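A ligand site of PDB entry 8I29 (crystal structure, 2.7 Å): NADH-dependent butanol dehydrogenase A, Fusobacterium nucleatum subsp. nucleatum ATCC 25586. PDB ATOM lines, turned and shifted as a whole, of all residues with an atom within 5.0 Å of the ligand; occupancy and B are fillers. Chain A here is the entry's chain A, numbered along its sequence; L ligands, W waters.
Water W1 lies within hydrogen-bond range of an oxygen (O2) of the ligand and the side-chain carboxylate of Glu 41.
N of Thr 143 is in hydrogen-bond range of O of Gly 101, 2.8 Å away. The side-chain hydroxyl (OG) of Ser 104 sits at hydrogen-bond distance from the side-chain carboxylate (OE1) of Glu 41 (3.2 Å). N of Ile 156 lies within hydrogen-bond range of OD2 of Asp 107 (3.0 Å). The backbone carbonyl oxygen (O) of Ser 149 sits at hydrogen-bond distance from the side-chain amino group (NZ) of Lys 110 (2.8 Å). The side-chain hydroxyl (OG) of Ser 152 sits at hydrogen-bond distance from the side-chain amino group (NZ) of Lys 110 (2.7 Å). The side-chain carboxylate (OD1) of Asp 107 lies within hydrogen-bond range of the side-chain hydroxyl (OG) of Ser 149 (2.6 Å). OG of Ser 152 lies within hydrogen-bond range of N of Ser 154, at 3.2 Å. The backbone carbonyl oxygen of Ser 154 lies within hydrogen-bond range of the side-chain amino group of Lys 110, 2.9 Å away.
O of Thr 143 is in hydrogen-bond range of N3 of the ligand, at 2.6 Å. A nitrogen (N2) of the ligand lies within hydrogen-bond range of the side-chain hydroxyl of Thr 143 (3.0 Å). N7 of the ligand sits at hydrogen-bond distance from OG of Ser 152 (2.8 Å). The side-chain hydroxyl of Ser 149 is in hydrogen-bond range of an oxygen (O14) of the ligand (3.2 Å). OG of Ser 104 sits at hydrogen-bond distance from O2 of the ligand, at 3.0 Å. N3 of the ligand lies within hydrogen-bond range of O of Val 184 (2.8 Å).
OD1 of Asp 107 sits close to O14 of the ligand. The backbone carbonyl oxygen (O) of Ser 154 sits close to an oxygen (O14) of the ligand (3.1 Å). Residues that only touch the ligand: Ala 103 (3.1 Å), Ala 147 (3.1 Å), Ile 144 (3.2 Å), Thr 187 (3.2 Å), Leu 192 (3.3 Å), Ile 156 (3.4 Å), Gly 102 (3.4 Å), Ile 188 (3.5 Å), Pro 75 (3.7 Å), Gly 146 (3.7 Å), Leu 50 (3.8 Å) and Leu 46 (3.8 Å). 19 residues have an atom within 4 Å of the ligand: Leu 46, Leu 50, Pro 75, Gly 102, Ala 103, Ser 104, Asp 107, Thr 143, Ile 144, Gly 146, Ala 147, Ser 149, Ser 152, Ser 154, Ile 156, Val 184, Thr 187, Ile 188 and Leu 192.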
ATOM      1  N   GLU A  41     -19.639  21.961  -1.497  1.00  0.00           N
ATOM      2  CA  GLU A  41     -19.728  22.678  -2.761  1.00  0.00           C
ATOM      3  C   GLU A  41     -20.063  24.131  -2.477  1.00  0.00           C
ATOM      4  O   GLU A  41     -20.814  24.440  -1.546  1.00  0.00           O
ATOM      5  CB  GLU A  41     -20.738  21.986  -3.670  1.00  0.00           C
ATOM      6  CG  GLU A  41     -20.513  22.268  -5.158  1.00  0.00           C
ATOM      7  CD  GLU A  41     -21.220  21.300  -6.087  1.00  0.00           C
ATOM      8  OE1 GLU A  41     -21.896  20.384  -5.569  1.00  0.00           O
ATOM      9  OE2 GLU A  41     -21.103  21.460  -7.338  1.00  0.00           O
ATOM     10  N   LEU A  46     -26.049  25.460   0.199  1.00  0.00           N
ATOM     11  CA  LEU A  46     -27.279  24.681   0.223  1.00  0.00           C
ATOM     12  C   LEU A  46     -27.200  23.598   1.312  1.00  0.00           C
ATOM     13  O   LEU A  46     -28.185  23.324   2.006  1.00  0.00           O
ATOM     14  CB  LEU A  46     -27.514  24.148  -1.199  1.00  0.00           C
ATOM     15  CG  LEU A  46     -27.629  25.229  -2.281  1.00  0.00           C
ATOM     16  CD1 LEU A  46     -27.938  24.623  -3.638  1.00  0.00           C
ATOM     17  CD2 LEU A  46     -28.678  26.279  -1.939  1.00  0.00           C
ATOM     18  N   LEU A  50     -30.141  23.431   4.322  1.00  0.00           N
ATOM     19  CA  LEU A  50     -30.890  22.238   4.700  1.00  0.00           C
ATOM     20  C   LEU A  50     -30.794  21.962   6.197  1.00  0.00           C
ATOM     21  O   LEU A  50     -31.703  21.384   6.764  1.00  0.00           O
ATOM     22  CB  LEU A  50     -30.364  21.030   3.896  1.00  0.00           C
ATOM     23  CG  LEU A  50     -30.430  21.162   2.376  1.00  0.00           C
ATOM     24  CD1 LEU A  50     -30.046  19.865   1.677  1.00  0.00           C
ATOM     25  CD2 LEU A  50     -31.813  21.599   1.907  1.00  0.00           C
ATOM     26  N   PRO A  75     -19.694  21.447  -9.889  1.00  0.00           N
ATOM     27  CA  PRO A  75     -20.118  20.129 -10.388  1.00  0.00           C
ATOM     28  C   PRO A  75     -19.053  19.272 -11.091  1.00  0.00           C
ATOM     29  O   PRO A  75     -19.103  18.045 -10.988  1.00  0.00           O
ATOM     30  CB  PRO A  75     -21.198  20.465 -11.427  1.00  0.00           C
ATOM     31  CG  PRO A  75     -21.717  21.812 -11.008  1.00  0.00           C
ATOM     32  CD  PRO A  75     -20.512  22.533 -10.449  1.00  0.00           C
ATOM     33  N   GLY A 101     -21.721  16.313   0.733  1.00  0.00           N
ATOM     34  CA  GLY A 101     -22.349  16.736  -0.508  1.00  0.00           C
ATOM     35  C   GLY A 101     -22.797  15.535  -1.354  1.00  0.00           C
ATOM     36  O   GLY A 101     -23.334  14.555  -0.828  1.00  0.00           O
ATOM     37  N   GLY A 102     -22.577  15.673  -2.674  1.00  0.00           N
ATOM     38  CA  GLY A 102     -22.712  14.595  -3.630  1.00  0.00           C
ATOM     39  C   GLY A 102     -21.408  14.374  -4.389  1.00  0.00           C
ATOM     40  O   GLY A 102     -20.367  14.919  -4.011  1.00  0.00           O
ATOM     41  N   ALA A 103     -21.471  13.614  -5.471  1.00  0.00           N
ATOM     42  CA  ALA A 103     -20.304  12.999  -6.079  1.00  0.00           C
ATOM     43  C   ALA A 103     -19.257  14.037  -6.469  1.00  0.00           C
ATOM     44  O   ALA A 103     -18.053  13.791  -6.379  1.00  0.00           O
ATOM     45  CB  ALA A 103     -20.731  12.179  -7.270  1.00  0.00           C
ATOM     46  N   SER A 104     -19.700  15.217  -6.890  1.00  0.00           N
ATOM     47  CA  SER A 104     -18.789  16.305  -7.178  1.00  0.00           C
ATOM     48  C   SER A 104     -17.825  16.601  -6.013  1.00  0.00           C
ATOM     49  O   SER A 104     -16.673  16.924  -6.255  1.00  0.00           O
ATOM     50  CB  SER A 104     -19.578  17.519  -7.575  1.00  0.00           C
ATOM     51  OG  SER A 104     -20.694  17.693  -6.696  1.00  0.00           O
ATOM     52  N   ASP A 107     -15.714  13.136  -5.061  1.00  0.00           N
ATOM     53  CA  ASP A 107     -14.612  12.888  -5.960  1.00  0.00           C
ATOM     54  C   ASP A 107     -13.449  13.817  -5.610  1.00  0.00           C
ATOM     55  O   ASP A 107     -12.303  13.393  -5.659  1.00  0.00           O
ATOM     56  CB  ASP A 107     -15.043  13.041  -7.428  1.00  0.00           C
ATOM     57  CG  ASP A 107     -15.836  11.868  -8.005  1.00  0.00           C
ATOM     58  OD1 ASP A 107     -16.156  10.911  -7.237  1.00  0.00           O
ATOM     59  OD2 ASP A 107     -16.124  11.915  -9.231  1.00  0.00           O
ATOM     60  N   LYS A 110     -11.813  12.436  -2.419  1.00  0.00           N
ATOM     61  CA  LYS A 110     -11.034  11.238  -2.681  1.00  0.00           C
ATOM     62  C   LYS A 110      -9.667  11.601  -3.278  1.00  0.00           C
ATOM     63  O   LYS A 110      -8.676  10.948  -2.955  1.00  0.00           O
ATOM     64  CB  LYS A 110     -11.756  10.331  -3.671  1.00  0.00           C
ATOM     65  CG  LYS A 110     -12.899   9.475  -3.128  1.00  0.00           C
ATOM     66  CD  LYS A 110     -13.491   8.615  -4.218  1.00  0.00           C
ATOM     67  CE  LYS A 110     -14.899   8.152  -3.936  1.00  0.00           C
ATOM     68  NZ  LYS A 110     -15.256   6.985  -4.781  1.00  0.00           N
ATOM     69  N   THR A 143     -25.799  13.804   0.197  1.00  0.00           N
ATOM     70  CA  THR A 143     -26.948  14.685   0.145  1.00  0.00           C
ATOM     71  C   THR A 143     -27.926  14.303  -0.956  1.00  0.00           C
ATOM     72  O   THR A 143     -29.021  14.839  -0.972  1.00  0.00           O
ATOM     73  CB  THR A 143     -26.516  16.142  -0.066  1.00  0.00           C
ATOM     74  OG1 THR A 143     -26.003  16.203  -1.388  1.00  0.00           O
ATOM     75  CG2 THR A 143     -25.507  16.597   0.960  1.00  0.00           C
ATOM     76  N   ILE A 144     -27.550  13.412  -1.894  1.00  0.00           N
ATOM     77  CA  ILE A 144     -28.467  12.974  -2.936  1.00  0.00           C
ATOM     78  C   ILE A 144     -28.035  11.627  -3.526  1.00  0.00           C
ATOM     79  O   ILE A 144     -26.942  11.552  -4.098  1.00  0.00           O
ATOM     80  CB  ILE A 144     -28.598  14.073  -4.020  1.00  0.00           C
ATOM     81  CG1 ILE A 144     -29.434  13.604  -5.208  1.00  0.00           C
ATOM     82  CG2 ILE A 144     -27.219  14.567  -4.441  1.00  0.00           C
ATOM     83  CD1 ILE A 144     -29.900  14.711  -6.140  1.00  0.00           C
ATOM     84  N   GLY A 146     -27.221   9.783  -5.885  1.00  0.00           N
ATOM     85  CA  GLY A 146     -26.853   9.813  -7.295  1.00  0.00           C
ATOM     86  C   GLY A 146     -26.134   8.531  -7.702  1.00  0.00           C
ATOM     87  O   GLY A 146     -26.686   7.436  -7.542  1.00  0.00           O
ATOM     88  N   ALA A 147     -24.886   8.665  -8.175  1.00  0.00           N
ATOM     89  CA  ALA A 147     -24.220   7.601  -8.905  1.00  0.00           C
ATOM     90  C   ALA A 147     -23.345   6.705  -8.025  1.00  0.00           C
ATOM     91  O   ALA A 147     -22.650   5.850  -8.546  1.00  0.00           O
ATOM     92  CB  ALA A 147     -23.409   8.229 -10.000  1.00  0.00           C
ATOM     93  N   GLY A 148     -23.380   6.867  -6.688  1.00  0.00           N
ATOM     94  CA  GLY A 148     -22.829   5.874  -5.770  1.00  0.00           C
ATOM     95  C   GLY A 148     -21.348   6.082  -5.430  1.00  0.00           C
ATOM     96  O   GLY A 148     -20.729   5.189  -4.854  1.00  0.00           O
ATOM     97  N   SER A 149     -20.789   7.269  -5.751  1.00  0.00           N
ATOM     98  CA  SER A 149     -19.376   7.565  -5.552  1.00  0.00           C
ATOM     99  C   SER A 149     -19.016   7.407  -4.072  1.00  0.00           C
ATOM    100  O   SER A 149     -17.861   7.185  -3.748  1.00  0.00           O
ATOM    101  CB  SER A 149     -19.014   8.940  -6.075  1.00  0.00           C
ATOM    102  OG  SER A 149     -17.607   9.195  -6.018  1.00  0.00           O
ATOM    103  N   SER A 152     -17.884   3.873  -4.303  1.00  0.00           N
ATOM    104  CA  SER A 152     -17.173   3.480  -5.507  1.00  0.00           C
ATOM    105  C   SER A 152     -15.668   3.499  -5.250  1.00  0.00           C
ATOM    106  O   SER A 152     -15.237   3.774  -4.140  1.00  0.00           O
ATOM    107  CB  SER A 152     -17.520   4.408  -6.651  1.00  0.00           C
ATOM    108  OG  SER A 152     -16.757   5.606  -6.583  1.00  0.00           O
ATOM    109  N   SER A 154     -13.754   5.210  -7.543  1.00  0.00           N
ATOM    110  CA  SER A 154     -13.505   6.103  -8.664  1.00  0.00           C
ATOM    111  C   SER A 154     -13.590   7.570  -8.235  1.00  0.00           C
ATOM    112  O   SER A 154     -14.355   7.964  -7.359  1.00  0.00           O
ATOM    113  CB  SER A 154     -14.488   5.809  -9.758  1.00  0.00           C
ATOM    114  OG  SER A 154     -14.760   4.408  -9.809  1.00  0.00           O
ATOM    115  N   SER A 155     -12.780   8.397  -8.903  1.00  0.00           N
ATOM    116  CA  SER A 155     -12.799   9.836  -8.722  1.00  0.00           C
ATOM    117  C   SER A 155     -12.569  10.488 -10.083  1.00  0.00           C
ATOM    118  O   SER A 155     -11.644  10.106 -10.813  1.00  0.00           O
ATOM    119  CB  SER A 155     -11.783  10.270  -7.699  1.00  0.00           C
ATOM    120  OG  SER A 155     -11.496  11.666  -7.814  1.00  0.00           O
ATOM    121  N   ILE A 156     -13.439  11.433 -10.419  1.00  0.00           N
ATOM    122  CA  ILE A 156     -13.476  12.044 -11.729  1.00  0.00           C
ATOM    123  C   ILE A 156     -13.177  13.508 -11.546  1.00  0.00           C
ATOM    124  O   ILE A 156     -13.958  14.213 -10.931  1.00  0.00           O
ATOM    125  CB  ILE A 156     -14.860  11.859 -12.398  1.00  0.00           C
ATOM    126  CG1 ILE A 156     -15.315  10.388 -12.393  1.00  0.00           C
ATOM    127  CG2 ILE A 156     -14.836  12.442 -13.809  1.00  0.00           C
ATOM    128  CD1 ILE A 156     -16.790  10.215 -12.613  1.00  0.00           C
ATOM    129  N   VAL A 184     -32.551  13.247   3.272  1.00  0.00           N
ATOM    130  CA  VAL A 184     -31.954  14.240   2.378  1.00  0.00           C
ATOM    131  C   VAL A 184     -32.684  14.269   1.039  1.00  0.00           C
ATOM    132  O   VAL A 184     -32.455  15.183   0.249  1.00  0.00           O
ATOM    133  CB  VAL A 184     -30.457  13.966   2.162  1.00  0.00           C
ATOM    134  CG1 VAL A 184     -29.730  13.848   3.491  1.00  0.00           C
ATOM    135  CG2 VAL A 184     -30.225  12.737   1.297  1.00  0.00           C
ATOM    136  N   CYS A 185     -33.510  13.250   0.782  1.00  0.00           N
ATOM    137  CA  CYS A 185     -34.299  13.154  -0.434  1.00  0.00           C
ATOM    138  C   CYS A 185     -35.380  14.251  -0.481  1.00  0.00           C
ATOM    139  O   CYS A 185     -35.678  14.778  -1.564  1.00  0.00           O
ATOM    140  CB  CYS A 185     -34.938  11.778  -0.538  1.00  0.00           C
ATOM    141  SG  CYS A 185     -33.802  10.443  -1.019  1.00  0.00           S
ATOM    142  N   THR A 187     -35.885  17.426   0.171  1.00  0.00           N
ATOM    143  CA  THR A 187     -35.745  18.782  -0.318  1.00  0.00           C
ATOM    144  C   THR A 187     -35.367  18.774  -1.805  1.00  0.00           C
ATOM    145  O   THR A 187     -35.292  19.848  -2.396  1.00  0.00           O
ATOM    146  CB  THR A 187     -34.734  19.525   0.553  1.00  0.00           C
ATOM    147  OG1 THR A 187     -34.456  20.740  -0.139  1.00  0.00           O
ATOM    148  CG2 THR A 187     -33.478  18.722   0.834  1.00  0.00           C
ATOM    149  N   ILE A 188     -35.109  17.596  -2.394  1.00  0.00           N
ATOM    150  CA  ILE A 188     -34.628  17.495  -3.766  1.00  0.00           C
ATOM    151  C   ILE A 188     -35.768  17.915  -4.698  1.00  0.00           C
ATOM    152  O   ILE A 188     -36.881  17.420  -4.559  1.00  0.00           O
ATOM    153  CB  ILE A 188     -34.126  16.063  -4.088  1.00  0.00           C
ATOM    154  CG1 ILE A 188     -32.867  15.705  -3.299  1.00  0.00           C
ATOM    155  CG2 ILE A 188     -33.908  15.848  -5.582  1.00  0.00           C
ATOM    156  CD1 ILE A 188     -32.448  14.270  -3.418  1.00  0.00           C
ATOM    157  N   PRO A 189     -35.544  18.821  -5.685  1.00  0.00           N
ATOM    158  CA  PRO A 189     -36.599  19.172  -6.635  1.00  0.00           C
ATOM    159  C   PRO A 189     -37.079  17.982  -7.466  1.00  0.00           C
ATOM    160  O   PRO A 189     -36.324  17.034  -7.767  1.00  0.00           O
ATOM    161  CB  PRO A 189     -36.006  20.261  -7.559  1.00  0.00           C
ATOM    162  CG  PRO A 189     -34.644  20.604  -6.948  1.00  0.00           C
ATOM    163  CD  PRO A 189     -34.266  19.477  -6.008  1.00  0.00           C
ATOM    164  N   LEU A 192     -35.349  16.565 -10.542  1.00  0.00           N
ATOM    165  CA  LEU A 192     -34.113  15.889 -10.170  1.00  0.00           C
ATOM    166  C   LEU A 192     -34.369  14.576  -9.461  1.00  0.00           C
ATOM    167  O   LEU A 192     -33.514  13.709  -9.550  1.00  0.00           O
ATOM    168  CB  LEU A 192     -33.242  16.779  -9.284  1.00  0.00           C
ATOM    169  CG  LEU A 192     -32.149  17.505 -10.046  1.00  0.00           C
ATOM    170  CD1 LEU A 192     -32.758  18.380 -11.144  1.00  0.00           C
ATOM    171  CD2 LEU A 192     -31.296  18.320  -9.090  1.00  0.00           C
HETATM  172  P1  LIG L   1     -24.501  16.493  -7.225  1.00  0.00           P
HETATM  173  O1  LIG L   1     -24.523  16.585  -5.733  1.00  0.00           O
HETATM  174  O2  LIG L   1     -23.196  16.540  -7.957  1.00  0.00           O
HETATM  175  O3  LIG L   1     -25.487  17.627  -7.791  1.00  0.00           O
HETATM  176  C1  LIG L   1     -26.902  17.387  -7.543  1.00  0.00           C
HETATM  177  C2  LIG L   1     -27.723  18.618  -7.823  1.00  0.00           C
HETATM  178  O4  LIG L   1     -28.861  18.646  -6.923  1.00  0.00           O
HETATM  179  C3  LIG L   1     -27.044  19.964  -7.551  1.00  0.00           C
HETATM  180  O5  LIG L   1     -27.786  20.963  -8.231  1.00  0.00           O
HETATM  181  C4  LIG L   1     -27.206  20.069  -6.030  1.00  0.00           C
HETATM  182  O6  LIG L   1     -27.255  21.413  -5.628  1.00  0.00           O
HETATM  183  C5  LIG L   1     -28.580  19.451  -5.801  1.00  0.00           C
HETATM  184  N1  LIG L   1     -28.726  18.641  -4.583  1.00  0.00           N
HETATM  185  C6  LIG L   1     -27.918  17.655  -4.070  1.00  0.00           C
HETATM  186  N2  LIG L   1     -28.376  17.128  -2.953  1.00  0.00           N
HETATM  187  C7  LIG L   1     -29.562  17.807  -2.721  1.00  0.00           C
HETATM  188  C8  LIG L   1     -30.525  17.721  -1.700  1.00  0.00           C
HETATM  189  N3  LIG L   1     -30.491  16.901  -0.665  1.00  0.00           N
HETATM  190  N4  LIG L   1     -31.573  18.579  -1.764  1.00  0.00           N
HETATM  191  C9  LIG L   1     -31.648  19.441  -2.785  1.00  0.00           C
HETATM  192  N5  LIG L   1     -30.809  19.589  -3.795  1.00  0.00           N
HETATM  193  C10 LIG L   1     -29.775  18.747  -3.708  1.00  0.00           C
HETATM  194  O7  LIG L   1     -25.252  15.130  -7.632  1.00  0.00           O
HETATM  195  P2  LIG L   1     -24.917  13.606  -8.080  1.00  0.00           P
HETATM  196  O8  LIG L   1     -25.976  13.121  -9.018  1.00  0.00           O
HETATM  197  O9  LIG L   1     -24.675  12.801  -6.852  1.00  0.00           O
HETATM  198  O10 LIG L   1     -23.531  13.845  -8.875  1.00  0.00           O
HETATM  199  C11 LIG L   1     -23.271  13.609 -10.296  1.00  0.00           C
HETATM  200  C12 LIG L   1     -21.775  13.410 -10.454  1.00  0.00           C
HETATM  201  O11 LIG L   1     -21.457  12.022 -10.232  1.00  0.00           O
HETATM  202  C13 LIG L   1     -21.124  13.771 -11.807  1.00  0.00           C
HETATM  203  O12 LIG L   1     -19.939  14.537 -11.584  1.00  0.00           O
HETATM  204  C14 LIG L   1     -20.778  12.394 -12.385  1.00  0.00           C
HETATM  205  O13 LIG L   1     -19.695  12.393 -13.309  1.00  0.00           O
HETATM  206  C15 LIG L   1     -20.368  11.714 -11.086  1.00  0.00           C
HETATM  207  N6  LIG L   1     -20.187  10.251 -11.074  1.00  0.00           N
HETATM  208  C16 LIG L   1     -19.193   9.709 -10.272  1.00  0.00           C
HETATM  209  C17 LIG L   1     -19.041   8.329 -10.196  1.00  0.00           C
HETATM  210  C18 LIG L   1     -17.946   7.755  -9.345  1.00  0.00           C
HETATM  211  O14 LIG L   1     -16.966   8.466  -9.048  1.00  0.00           O
HETATM  212  N7  LIG L   1     -18.140   6.550  -8.834  1.00  0.00           N
HETATM  213  C19 LIG L   1     -19.843   7.510 -10.974  1.00  0.00           C
HETATM  214  C20 LIG L   1     -20.830   8.065 -11.775  1.00  0.00           C
HETATM  215  C21 LIG L   1     -20.995   9.426 -11.807  1.00  0.00           C
HETATM  216  O   HOH W   1     -22.835  19.426  -8.902  1.00  0.00           O
